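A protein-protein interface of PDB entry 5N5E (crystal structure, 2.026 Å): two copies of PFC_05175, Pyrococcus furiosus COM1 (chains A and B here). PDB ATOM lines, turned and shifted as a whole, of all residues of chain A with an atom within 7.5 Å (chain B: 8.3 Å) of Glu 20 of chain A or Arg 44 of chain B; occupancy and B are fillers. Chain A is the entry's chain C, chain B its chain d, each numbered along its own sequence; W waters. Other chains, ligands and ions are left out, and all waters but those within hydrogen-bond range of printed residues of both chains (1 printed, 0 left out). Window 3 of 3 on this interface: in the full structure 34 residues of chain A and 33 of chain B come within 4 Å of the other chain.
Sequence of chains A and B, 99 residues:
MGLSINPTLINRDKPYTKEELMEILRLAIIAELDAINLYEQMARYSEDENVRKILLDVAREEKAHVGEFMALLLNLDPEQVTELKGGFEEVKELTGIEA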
ATOM      1  N   ARG A  12      -0.429   8.976  10.660  1.00  0.00           N
ATOM      2  CA  ARG A  12      -0.291   8.055  11.781  1.00  0.00           C
ATOM      3  C   ARG A  12      -1.459   8.247  12.742  1.00  0.00           C
ATOM      4  O   ARG A  12      -1.825   9.380  13.068  1.00  0.00           O
ATOM      5  CB  ARG A  12       1.039   8.297  12.494  1.00  0.00           C
ATOM      6  CG  ARG A  12       1.195   7.550  13.806  1.00  0.00           C
ATOM      7  CD  ARG A  12       2.659   7.438  14.207  1.00  0.00           C
ATOM      8  NE  ARG A  12       2.843   6.541  15.345  1.00  0.00           N
ATOM      9  CZ  ARG A  12       3.963   5.875  15.609  1.00  0.00           C
ATOM     10  NH1 ARG A  12       4.022   5.080  16.668  1.00  0.00           N
ATOM     11  NH2 ARG A  12       5.023   5.996  14.818  1.00  0.00           N
ATOM     12  N   LYS A  14      -1.666   6.139  15.737  1.00  0.00           N
ATOM     13  CA  LYS A  14      -1.339   5.322  16.896  1.00  0.00           C
ATOM     14  C   LYS A  14      -0.199   5.967  17.669  1.00  0.00           C
ATOM     15  O   LYS A  14       0.657   6.635  17.076  1.00  0.00           O
ATOM     16  CB  LYS A  14      -0.948   3.894  16.489  1.00  0.00           C
ATOM     17  CG  LYS A  14       0.174   3.822  15.476  1.00  0.00           C
ATOM     18  CD  LYS A  14       0.251   2.446  14.834  1.00  0.00           C
ATOM     19  CE  LYS A  14       1.331   2.388  13.764  1.00  0.00           C
ATOM     20  NZ  LYS A  14       1.123   3.405  12.692  1.00  0.00           N
ATOM     21  N   PRO A  15      -0.161   5.784  18.987  1.00  0.00           N
ATOM     22  CA  PRO A  15       0.849   6.472  19.796  1.00  0.00           C
ATOM     23  C   PRO A  15       2.229   5.854  19.639  1.00  0.00           C
ATOM     24  O   PRO A  15       2.394   4.719  19.183  1.00  0.00           O
ATOM     25  CB  PRO A  15       0.328   6.306  21.227  1.00  0.00           C
ATOM     26  CG  PRO A  15      -0.469   5.050  21.184  1.00  0.00           C
ATOM     27  CD  PRO A  15      -1.091   4.999  19.819  1.00  0.00           C
ATOM     28  N   TYR A  16       3.231   6.630  20.042  1.00  0.00           N
ATOM     29  CA  TYR A  16       4.612   6.176  19.982  1.00  0.00           C
ATOM     30  C   TYR A  16       4.817   4.963  20.882  1.00  0.00           C
ATOM     31  O   TYR A  16       4.294   4.900  21.997  1.00  0.00           O
ATOM     32  CB  TYR A  16       5.559   7.295  20.420  1.00  0.00           C
ATOM     33  CG  TYR A  16       5.606   8.498  19.501  1.00  0.00           C
ATOM     34  CD1 TYR A  16       5.597   8.353  18.120  1.00  0.00           C
ATOM     35  CD2 TYR A  16       5.667   9.784  20.024  1.00  0.00           C
ATOM     36  CE1 TYR A  16       5.644   9.458  17.285  1.00  0.00           C
ATOM     37  CE2 TYR A  16       5.717  10.891  19.202  1.00  0.00           C
ATOM     38  CZ  TYR A  16       5.705  10.724  17.832  1.00  0.00           C
ATOM     39  OH  TYR A  16       5.753  11.829  17.013  1.00  0.00           O
ATOM     40  N   THR A  17       5.590   3.999  20.390  1.00  0.00           N
ATOM     41  CA  THR A  17       6.078   2.920  21.234  1.00  0.00           C
ATOM     42  C   THR A  17       7.164   3.455  22.168  1.00  0.00           C
ATOM     43  O   THR A  17       7.625   4.592  22.037  1.00  0.00           O
ATOM     44  CB  THR A  17       6.625   1.774  20.383  1.00  0.00           C
ATOM     45  OG1 THR A  17       7.778   2.224  19.660  1.00  0.00           O
ATOM     46  CG2 THR A  17       5.574   1.274  19.402  1.00  0.00           C
ATOM     47  N   LYS A  18       7.581   2.623  23.127  1.00  0.00           N
ATOM     48  CA  LYS A  18       8.602   3.075  24.067  1.00  0.00           C
ATOM     49  C   LYS A  18       9.903   3.408  23.348  1.00  0.00           C
ATOM     50  O   LYS A  18      10.611   4.341  23.742  1.00  0.00           O
ATOM     51  CB  LYS A  18       8.841   2.026  25.158  1.00  0.00           C
ATOM     52  CG  LYS A  18       9.669   0.808  24.749  1.00  0.00           C
ATOM     53  CD  LYS A  18      10.323   0.161  25.962  1.00  0.00           C
ATOM     54  CE  LYS A  18      11.401  -0.829  25.552  1.00  0.00           C
ATOM     55  NZ  LYS A  18      12.284  -1.200  26.694  1.00  0.00           N
ATOM     56  N   GLU A  19      10.232   2.662  22.291  1.00  0.00           N
ATOM     57  CA  GLU A  19      11.448   2.938  21.536  1.00  0.00           C
ATOM     58  C   GLU A  19      11.306   4.220  20.727  1.00  0.00           C
ATOM     59  O   GLU A  19      12.255   5.006  20.621  1.00  0.00           O
ATOM     60  CB  GLU A  19      11.770   1.755  20.624  1.00  0.00           C
ATOM     61  CG  GLU A  19      13.199   1.723  20.113  1.00  0.00           C
ATOM     62  CD  GLU A  19      13.502   0.465  19.319  1.00  0.00           C
ATOM     63  OE1 GLU A  19      12.595  -0.030  18.616  1.00  0.00           O
ATOM     64  OE2 GLU A  19      14.644  -0.036  19.404  1.00  0.00           O
ATOM     65  N   GLU A  20      10.125   4.449  20.151  1.00  0.00           N
ATOM     66  CA  GLU A  20       9.888   5.683  19.412  1.00  0.00           C
ATOM     67  C   GLU A  20       9.908   6.900  20.330  1.00  0.00           C
ATOM     68  O   GLU A  20      10.316   7.986  19.903  1.00  0.00           O
ATOM     69  CB  GLU A  20       8.558   5.591  18.664  1.00  0.00           C
ATOM     70  CG  GLU A  20       8.589   4.627  17.482  1.00  0.00           C
ATOM     71  CD  GLU A  20       7.218   4.385  16.888  1.00  0.00           C
ATOM     72  OE1 GLU A  20       6.221   4.453  17.639  1.00  0.00           O
ATOM     73  OE2 GLU A  20       7.133   4.141  15.665  1.00  0.00           O
ATOM     74  N   LEU A  21       9.479   6.742  21.586  1.00  0.00           N
ATOM     75  CA  LEU A  21       9.555   7.849  22.535  1.00  0.00           C
ATOM     76  C   LEU A  21      10.998   8.262  22.778  1.00  0.00           C
ATOM     77  O   LEU A  21      11.302   9.456  22.889  1.00  0.00           O
ATOM     78  CB  LEU A  21       8.892   7.463  23.858  1.00  0.00           C
ATOM     79  CG  LEU A  21       7.385   7.672  24.000  1.00  0.00           C
ATOM     80  CD1 LEU A  21       6.932   7.167  25.363  1.00  0.00           C
ATOM     81  CD2 LEU A  21       7.000   9.136  23.823  1.00  0.00           C
ATOM     82  N   MET A  22      11.903   7.290  22.888  1.00  0.00           N
ATOM     83  CA  MET A  22      13.315   7.624  23.016  1.00  0.00           C
ATOM     84  C   MET A  22      13.806   8.374  21.786  1.00  0.00           C
ATOM     85  O   MET A  22      14.638   9.281  21.902  1.00  0.00           O
ATOM     86  CB  MET A  22      14.137   6.353  23.233  1.00  0.00           C
ATOM     87  CG  MET A  22      13.735   5.554  24.470  1.00  0.00           C
ATOM     88  SD  MET A  22      14.289   3.835  24.421  1.00  0.00           S
ATOM     89  CE  MET A  22      16.059   4.027  24.580  1.00  0.00           C
ATOM     90  N   GLU A  23      13.278   8.033  20.609  1.00  0.00           N
ATOM     91  CA  GLU A  23      13.763   8.636  19.372  1.00  0.00           C
ATOM     92  C   GLU A  23      13.281  10.074  19.226  1.00  0.00           C
ATOM     93  O   GLU A  23      14.034  10.937  18.760  1.00  0.00           O
ATOM     94  CB  GLU A  23      13.328   7.782  18.182  1.00  0.00           C
ATOM     95  CG  GLU A  23      14.069   6.454  18.115  1.00  0.00           C
ATOM     96  CD  GLU A  23      13.450   5.465  17.148  1.00  0.00           C
ATOM     97  OE1 GLU A  23      12.626   5.877  16.302  1.00  0.00           O
ATOM     98  OE2 GLU A  23      13.789   4.267  17.242  1.00  0.00           O
ATOM     99  N   ILE A  24      12.042  10.365  19.631  1.00  0.00           N
ATOM    100  CA  ILE A  24      11.558  11.736  19.502  1.00  0.00           C
ATOM    101  C   ILE A  24      12.236  12.633  20.527  1.00  0.00           C
ATOM    102  O   ILE A  24      12.399  13.836  20.295  1.00  0.00           O
ATOM    103  CB  ILE A  24      10.021  11.802  19.622  1.00  0.00           C
ATOM    104  CG1 ILE A  24       9.557  11.367  21.012  1.00  0.00           C
ATOM    105  CG2 ILE A  24       9.364  10.938  18.553  1.00  0.00           C
ATOM    106  CD1 ILE A  24       9.237  12.522  21.936  1.00  0.00           C
ATOM    107  N   LEU A  25      12.658  12.075  21.664  1.00  0.00           N
ATOM    108  CA  LEU A  25      13.422  12.865  22.622  1.00  0.00           C
ATOM    109  C   LEU A  25      14.795  13.221  22.068  1.00  0.00           C
ATOM    110  O   LEU A  25      15.267  14.349  22.246  1.00  0.00           O
ATOM    111  CB  LEU A  25      13.549  12.115  23.949  1.00  0.00           C
ATOM    112  CG  LEU A  25      12.282  12.037  24.809  1.00  0.00           C
ATOM    113  CD1 LEU A  25      12.497  11.115  25.997  1.00  0.00           C
ATOM    114  CD2 LEU A  25      11.859  13.420  25.289  1.00  0.00           C
ATOM    115  N   ARG A  26      15.450  12.278  21.389  1.00  0.00           N
ATOM    116  CA  ARG A  26      16.714  12.595  20.730  1.00  0.00           C
ATOM    117  C   ARG A  26      16.503  13.612  19.615  1.00  0.00           C
ATOM    118  O   ARG A  26      17.328  14.514  19.421  1.00  0.00           O
ATOM    119  CB  ARG A  26      17.358  11.321  20.181  1.00  0.00           C
ATOM    120  CG  ARG A  26      17.653  10.275  21.245  1.00  0.00           C
ATOM    121  CD  ARG A  26      18.587   9.185  20.741  1.00  0.00           C
ATOM    122  NE  ARG A  26      18.600   8.025  21.634  1.00  0.00           N
ATOM    123  CZ  ARG A  26      17.831   6.948  21.496  1.00  0.00           C
ATOM    124  NH1 ARG A  26      17.924   5.956  22.370  1.00  0.00           N
ATOM    125  NH2 ARG A  26      16.968   6.851  20.494  1.00  0.00           N
ATOM    126  N   ASN B  37      19.333   7.025  16.568  1.00  0.00           N
ATOM    127  CA  ASN B  37      17.981   6.811  16.061  1.00  0.00           C
ATOM    128  C   ASN B  37      17.986   5.896  14.842  1.00  0.00           C
ATOM    129  O   ASN B  37      17.117   5.028  14.705  1.00  0.00           O
ATOM    130  CB  ASN B  37      17.321   8.146  15.724  1.00  0.00           C
ATOM    131  CG  ASN B  37      16.706   8.814  16.939  1.00  0.00           C
ATOM    132  OD1 ASN B  37      16.914   8.378  18.071  1.00  0.00           O
ATOM    133  ND2 ASN B  37      15.939   9.874  16.710  1.00  0.00           N
ATOM    134  N   LEU B  38      18.952   6.082  13.939  1.00  0.00           N
ATOM    135  CA  LEU B  38      19.007   5.258  12.734  1.00  0.00           C
ATOM    136  C   LEU B  38      19.191   3.787  13.087  1.00  0.00           C
ATOM    137  O   LEU B  38      18.464   2.919  12.590  1.00  0.00           O
ATOM    138  CB  LEU B  38      20.141   5.732  11.825  1.00  0.00           C
ATOM    139  CG  LEU B  38      20.277   4.996  10.490  1.00  0.00           C
ATOM    140  CD1 LEU B  38      19.084   5.303   9.595  1.00  0.00           C
ATOM    141  CD2 LEU B  38      21.583   5.358   9.794  1.00  0.00           C
ATOM    142  N   TYR B  39      20.172   3.485  13.939  1.00  0.00           N
ATOM    143  CA  TYR B  39      20.469   2.092  14.251  1.00  0.00           C
ATOM    144  C   TYR B  39      19.385   1.482  15.127  1.00  0.00           C
ATOM    145  O   TYR B  39      19.024   0.312  14.952  1.00  0.00           O
ATOM    146  CB  TYR B  39      21.837   1.992  14.923  1.00  0.00           C
ATOM    147  CG  TYR B  39      22.969   2.498  14.055  1.00  0.00           C
ATOM    148  CD1 TYR B  39      22.886   2.444  12.669  1.00  0.00           C
ATOM    149  CD2 TYR B  39      24.120   3.030  14.620  1.00  0.00           C
ATOM    150  CE1 TYR B  39      23.914   2.902  11.873  1.00  0.00           C
ATOM    151  CE2 TYR B  39      25.155   3.492  13.828  1.00  0.00           C
ATOM    152  CZ  TYR B  39      25.047   3.423  12.457  1.00  0.00           C
ATOM    153  OH  TYR B  39      26.071   3.882  11.660  1.00  0.00           O
ATOM    154  N   GLU B  40      18.851   2.258  16.072  1.00  0.00           N
ATOM    155  CA  GLU B  40      17.738   1.778  16.883  1.00  0.00           C
ATOM    156  C   GLU B  40      16.535   1.443  16.007  1.00  0.00           C
ATOM    157  O   GLU B  40      15.837   0.450  16.248  1.00  0.00           O
ATOM    158  CB  GLU B  40      17.377   2.830  17.933  1.00  0.00           C
ATOM    159  CG  GLU B  40      16.535   2.311  19.085  1.00  0.00           C
ATOM    160  CD  GLU B  40      16.316   3.358  20.167  1.00  0.00           C
ATOM    161  OE1 GLU B  40      15.521   4.296  19.946  1.00  0.00           O
ATOM    162  OE2 GLU B  40      16.950   3.246  21.240  1.00  0.00           O
ATOM    163  N   GLN B  41      16.285   2.253  14.974  1.00  0.00           N
ATOM    164  CA  GLN B  41      15.207   1.959  14.036  1.00  0.00           C
ATOM    165  C   GLN B  41      15.516   0.716  13.210  1.00  0.00           C
ATOM    166  O   GLN B  41      14.644  -0.137  13.010  1.00  0.00           O
ATOM    167  CB  GLN B  41      14.966   3.166  13.126  1.00  0.00           C
ATOM    168  CG  GLN B  41      14.280   4.329  13.823  1.00  0.00           C
ATOM    169  CD  GLN B  41      14.301   5.609  13.004  1.00  0.00           C
ATOM    170  OE1 GLN B  41      14.785   5.633  11.871  1.00  0.00           O
ATOM    171  NE2 GLN B  41      13.765   6.681  13.575  1.00  0.00           N
ATOM    172  N   MET B  42      16.749   0.600  12.712  1.00  0.00           N
ATOM    173  CA  MET B  42      17.138  -0.589  11.960  1.00  0.00           C
ATOM    174  C   MET B  42      16.996  -1.846  12.811  1.00  0.00           C
ATOM    175  O   MET B  42      16.479  -2.870  12.348  1.00  0.00           O
ATOM    176  CB  MET B  42      18.575  -0.440  11.460  1.00  0.00           C
ATOM    177  CG  MET B  42      18.746   0.592  10.357  1.00  0.00           C
ATOM    178  SD  MET B  42      20.480   0.861   9.943  1.00  0.00           S
ATOM    179  CE  MET B  42      20.319   1.910   8.502  1.00  0.00           C
ATOM    180  N   ALA B  43      17.465  -1.790  14.060  1.00  0.00           N
ATOM    181  CA  ALA B  43      17.383  -2.951  14.939  1.00  0.00           C
ATOM    182  C   ALA B  43      15.940  -3.369  15.181  1.00  0.00           C
ATOM    183  O   ALA B  43      15.665  -4.552  15.411  1.00  0.00           O
ATOM    184  CB  ALA B  43      18.074  -2.650  16.268  1.00  0.00           C
ATOM    185  N   ARG B  44      15.008  -2.415  15.135  1.00  0.00           N
ATOM    186  CA  ARG B  44      13.604  -2.724  15.379  1.00  0.00           C
ATOM    187  C   ARG B  44      13.056  -3.688  14.332  1.00  0.00           C
ATOM    188  O   ARG B  44      12.300  -4.610  14.663  1.00  0.00           O
ATOM    189  CB  ARG B  44      12.795  -1.425  15.403  1.00  0.00           C
ATOM    190  CG  ARG B  44      11.284  -1.594  15.352  1.00  0.00           C
ATOM    191  CD  ARG B  44      10.592  -0.238  15.382  1.00  0.00           C
ATOM    192  NE  ARG B  44       9.177  -0.327  15.030  1.00  0.00           N
ATOM    193  CZ  ARG B  44       8.364   0.720  14.924  1.00  0.00           C
ATOM    194  NH1 ARG B  44       7.091   0.541  14.598  1.00  0.00           N
ATOM    195  NH2 ARG B  44       8.820   1.949  15.140  1.00  0.00           N
ATOM    196  N   TYR B  45      13.427  -3.500  13.068  1.00  0.00           N
ATOM    197  CA  TYR B  45      12.862  -4.268  11.967  1.00  0.00           C
ATOM    198  C   TYR B  45      13.771  -5.398  11.497  1.00  0.00           C
ATOM    199  O   TYR B  45      13.472  -6.033  10.482  1.00  0.00           O
ATOM    200  CB  TYR B  45      12.544  -3.340  10.793  1.00  0.00           C
ATOM    201  CG  TYR B  45      11.509  -2.285  11.110  1.00  0.00           C
ATOM    202  CD1 TYR B  45      10.167  -2.615  11.228  1.00  0.00           C
ATOM    203  CD2 TYR B  45      11.876  -0.958  11.285  1.00  0.00           C
ATOM    204  CE1 TYR B  45       9.218  -1.654  11.515  1.00  0.00           C
ATOM    205  CE2 TYR B  45      10.933   0.012  11.571  1.00  0.00           C
ATOM    206  CZ  TYR B  45       9.607  -0.342  11.684  1.00  0.00           C
ATOM    207  OH  TYR B  45       8.666   0.618  11.969  1.00  0.00           O
ATOM    208  N   SER B  46      14.862  -5.667  12.209  1.00  0.00           N
ATOM    209  CA  SER B  46      15.805  -6.717  11.832  1.00  0.00           C
ATOM    210  C   SER B  46      15.492  -7.966  12.649  1.00  0.00           C
ATOM    211  O   SER B  46      15.834  -8.047  13.832  1.00  0.00           O
ATOM    212  CB  SER B  46      17.242  -6.258  12.054  1.00  0.00           C
ATOM    213  OG  SER B  46      17.548  -5.136  11.248  1.00  0.00           O
ATOM    214  N   GLU B  47      14.841  -8.943  12.017  1.00  0.00           N
ATOM    215  CA  GLU B  47      14.633 -10.236  12.656  1.00  0.00           C
ATOM    216  C   GLU B  47      15.876 -11.113  12.618  1.00  0.00           C
ATOM    217  O   GLU B  47      15.924 -12.122  13.329  1.00  0.00           O
ATOM    218  CB  GLU B  47      13.462 -10.973  12.001  1.00  0.00           C
ATOM    219  CG  GLU B  47      12.126 -10.718  12.685  1.00  0.00           C
ATOM    220  CD  GLU B  47      10.996 -11.537  12.092  1.00  0.00           C
ATOM    221  OE1 GLU B  47      11.128 -11.988  10.935  1.00  0.00           O
ATOM    222  OE2 GLU B  47       9.976 -11.734  12.787  1.00  0.00           O
ATOM    223  N   ASP B  48      16.874 -10.758  11.810  1.00  0.00           N
ATOM    224  CA  ASP B  48      18.181 -11.401  11.873  1.00  0.00           C
ATOM    225  C   ASP B  48      18.853 -11.008  13.182  1.00  0.00           C
ATOM    226  O   ASP B  48      19.274  -9.858  13.352  1.00  0.00           O
ATOM    227  CB  ASP B  48      19.022 -10.991  10.666  1.00  0.00           C
ATOM    228  CG  ASP B  48      20.373 -11.686  10.618  1.00  0.00           C
ATOM    229  OD1 ASP B  48      21.031 -11.810  11.672  1.00  0.00           O
ATOM    230  OD2 ASP B  48      20.781 -12.107   9.515  1.00  0.00           O
ATOM    231  N   ARG B  52      20.761  -7.493  14.393  1.00  0.00           N
ATOM    232  CA  ARG B  52      20.212  -6.709  15.495  1.00  0.00           C
ATOM    233  C   ARG B  52      21.240  -6.524  16.605  1.00  0.00           C
ATOM    234  O   ARG B  52      21.325  -5.449  17.210  1.00  0.00           O
ATOM    235  CB  ARG B  52      18.949  -7.380  16.038  1.00  0.00           C
ATOM    236  CG  ARG B  52      18.424  -6.770  17.333  1.00  0.00           C
ATOM    237  CD  ARG B  52      17.109  -7.400  17.763  1.00  0.00           C
ATOM    238  NE  ARG B  52      16.015  -7.063  16.858  1.00  0.00           N
ATOM    239  CZ  ARG B  52      14.750  -7.430  17.041  1.00  0.00           C
ATOM    240  NH1 ARG B  52      13.823  -7.074  16.162  1.00  0.00           N
ATOM    241  NH2 ARG B  52      14.407  -8.152  18.100  1.00  0.00           N
ATOM    242  N   LEU B  55      23.850  -3.847  15.557  1.00  0.00           N
ATOM    243  CA  LEU B  55      23.226  -2.528  15.517  1.00  0.00           C
ATOM    244  C   LEU B  55      23.079  -1.952  16.920  1.00  0.00           C
ATOM    245  O   LEU B  55      23.394  -0.780  17.159  1.00  0.00           O
ATOM    246  CB  LEU B  55      21.862  -2.617  14.830  1.00  0.00           C
ATOM    247  CG  LEU B  55      21.861  -2.698  13.301  1.00  0.00           C
ATOM    248  CD1 LEU B  55      20.502  -3.160  12.787  1.00  0.00           C
ATOM    249  CD2 LEU B  55      22.230  -1.350  12.694  1.00  0.00           C
ATOM    250  N   LEU B  56      22.609  -2.767  17.866  1.00  0.00           N
ATOM    251  CA  LEU B  56      22.426  -2.288  19.230  1.00  0.00           C
ATOM    252  C   LEU B  56      23.761  -2.040  19.920  1.00  0.00           C
ATOM    253  O   LEU B  56      23.865  -1.132  20.752  1.00  0.00           O
ATOM    254  CB  LEU B  56      21.592  -3.285  20.032  1.00  0.00           C
ATOM    255  CG  LEU B  56      20.150  -3.486  19.562  1.00  0.00           C
ATOM    256  CD1 LEU B  56      19.480  -4.587  20.365  1.00  0.00           C
ATOM    257  CD2 LEU B  56      19.353  -2.193  19.668  1.00  0.00           C
HETATM  258  O   HOH W   1      11.519   2.936  15.993  1.00  0.00           O
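Among the printed residues, pairs that only touch across the chains: Glu 19 of chain A with Arg 44 of chain B and Met 22 of chain A with Glu 40 of chain B.
O of Arg 44 of chain B lies within hydrogen-bond range of NH1 of Arg 52 of chain B, at 3.3 Å. NH1 of Arg 44 of chain B lies close to OH of Tyr 45 of chain B (3.1 Å). The side-chain carboxylate (OE1) of Glu 20 of chain A is in salt-bridge range of the guanidinium group (NH1) of Arg 12 of chain A. The side-chain carboxylate (OE1) of Glu 20 of chain A lies within hydrogen-bond range of the backbone NH (N) of Thr 17 of chain A.
Of chain B, only Arg 44 comes within 4 Å of Glu 20 of chain A. Arg 44 of chain B touches just these residues of chain A: Glu 19 and Glu 20. No residue of chain A comes within 4 Å of Ala 43 of chain B. Of the printed residues of chain B, Glu 23 of chain A touches Asn 37, Glu 40 and Gln 41. Of the printed residues of chain A, Gln 41 of chain B touches Glu 23 (3.1 Å). Lys 18 of chain A touches none of the printed residues of chain B. Glu 47 of chain B touches none of the printed residues of chain A. The nearest residue of chain B that does not touch Glu 20 of chain A is Tyr 45 of chain B (5.3 Å).
Hydrophobic or aromatic side chains of chain A within 4 Å of the printed part of chain B: Met 22. Among the printed residues, 9 pairs touch across the chains. Among the printed residues, Asp or Glu carboxylates within 4 Å of a Lys or Arg side-chain nitrogen of the other chain: Glu 20 of chain A with Arg 44 of chain B (2.8 Å) and Arg 26 of chain A with Glu 40 of chain B (3.0 Å).
Water W1 bridges OE2 of Glu 23 of chain A (2.9 Å) and NH2 of Arg 44 of chain B (3.0 Å).
The side-chain carboxylate (OE1) of Glu 40 of chain B sits close to the side-chain carboxylate (OE2) of Glu 23 of chain A (3.2 Å). The side-chain carboxylate (OE2) of Glu 20 of chain A lies within salt-bridge range of the guanidinium group (NH2) of Arg 44 of chain B (2.8 Å). O of Glu 40 of chain B sits close to OE2 of Glu 19 of chain A (3.4 Å). OE1 of Glu 23 of chain A is in hydrogen-bond range of NE2 of Gln 41 of chain B (3.1 Å). NH2 of Arg 26 of chain A sits at hydrogen-bond distance from OD1 of Asn 37 of chain B (2.9 Å). The backbone carbonyl oxygen (O) of Glu 23 of chain A sits at hydrogen-bond distance from the side-chain amide nitrogen (ND2) of Asn 37 of chain B. The guanidinium group (NH2) of Arg 26 of chain A lies within salt-bridge range of the side-chain carboxylate (OE1) of Glu 40 of chain B (3.0 Å).
No position is printed for both chains.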
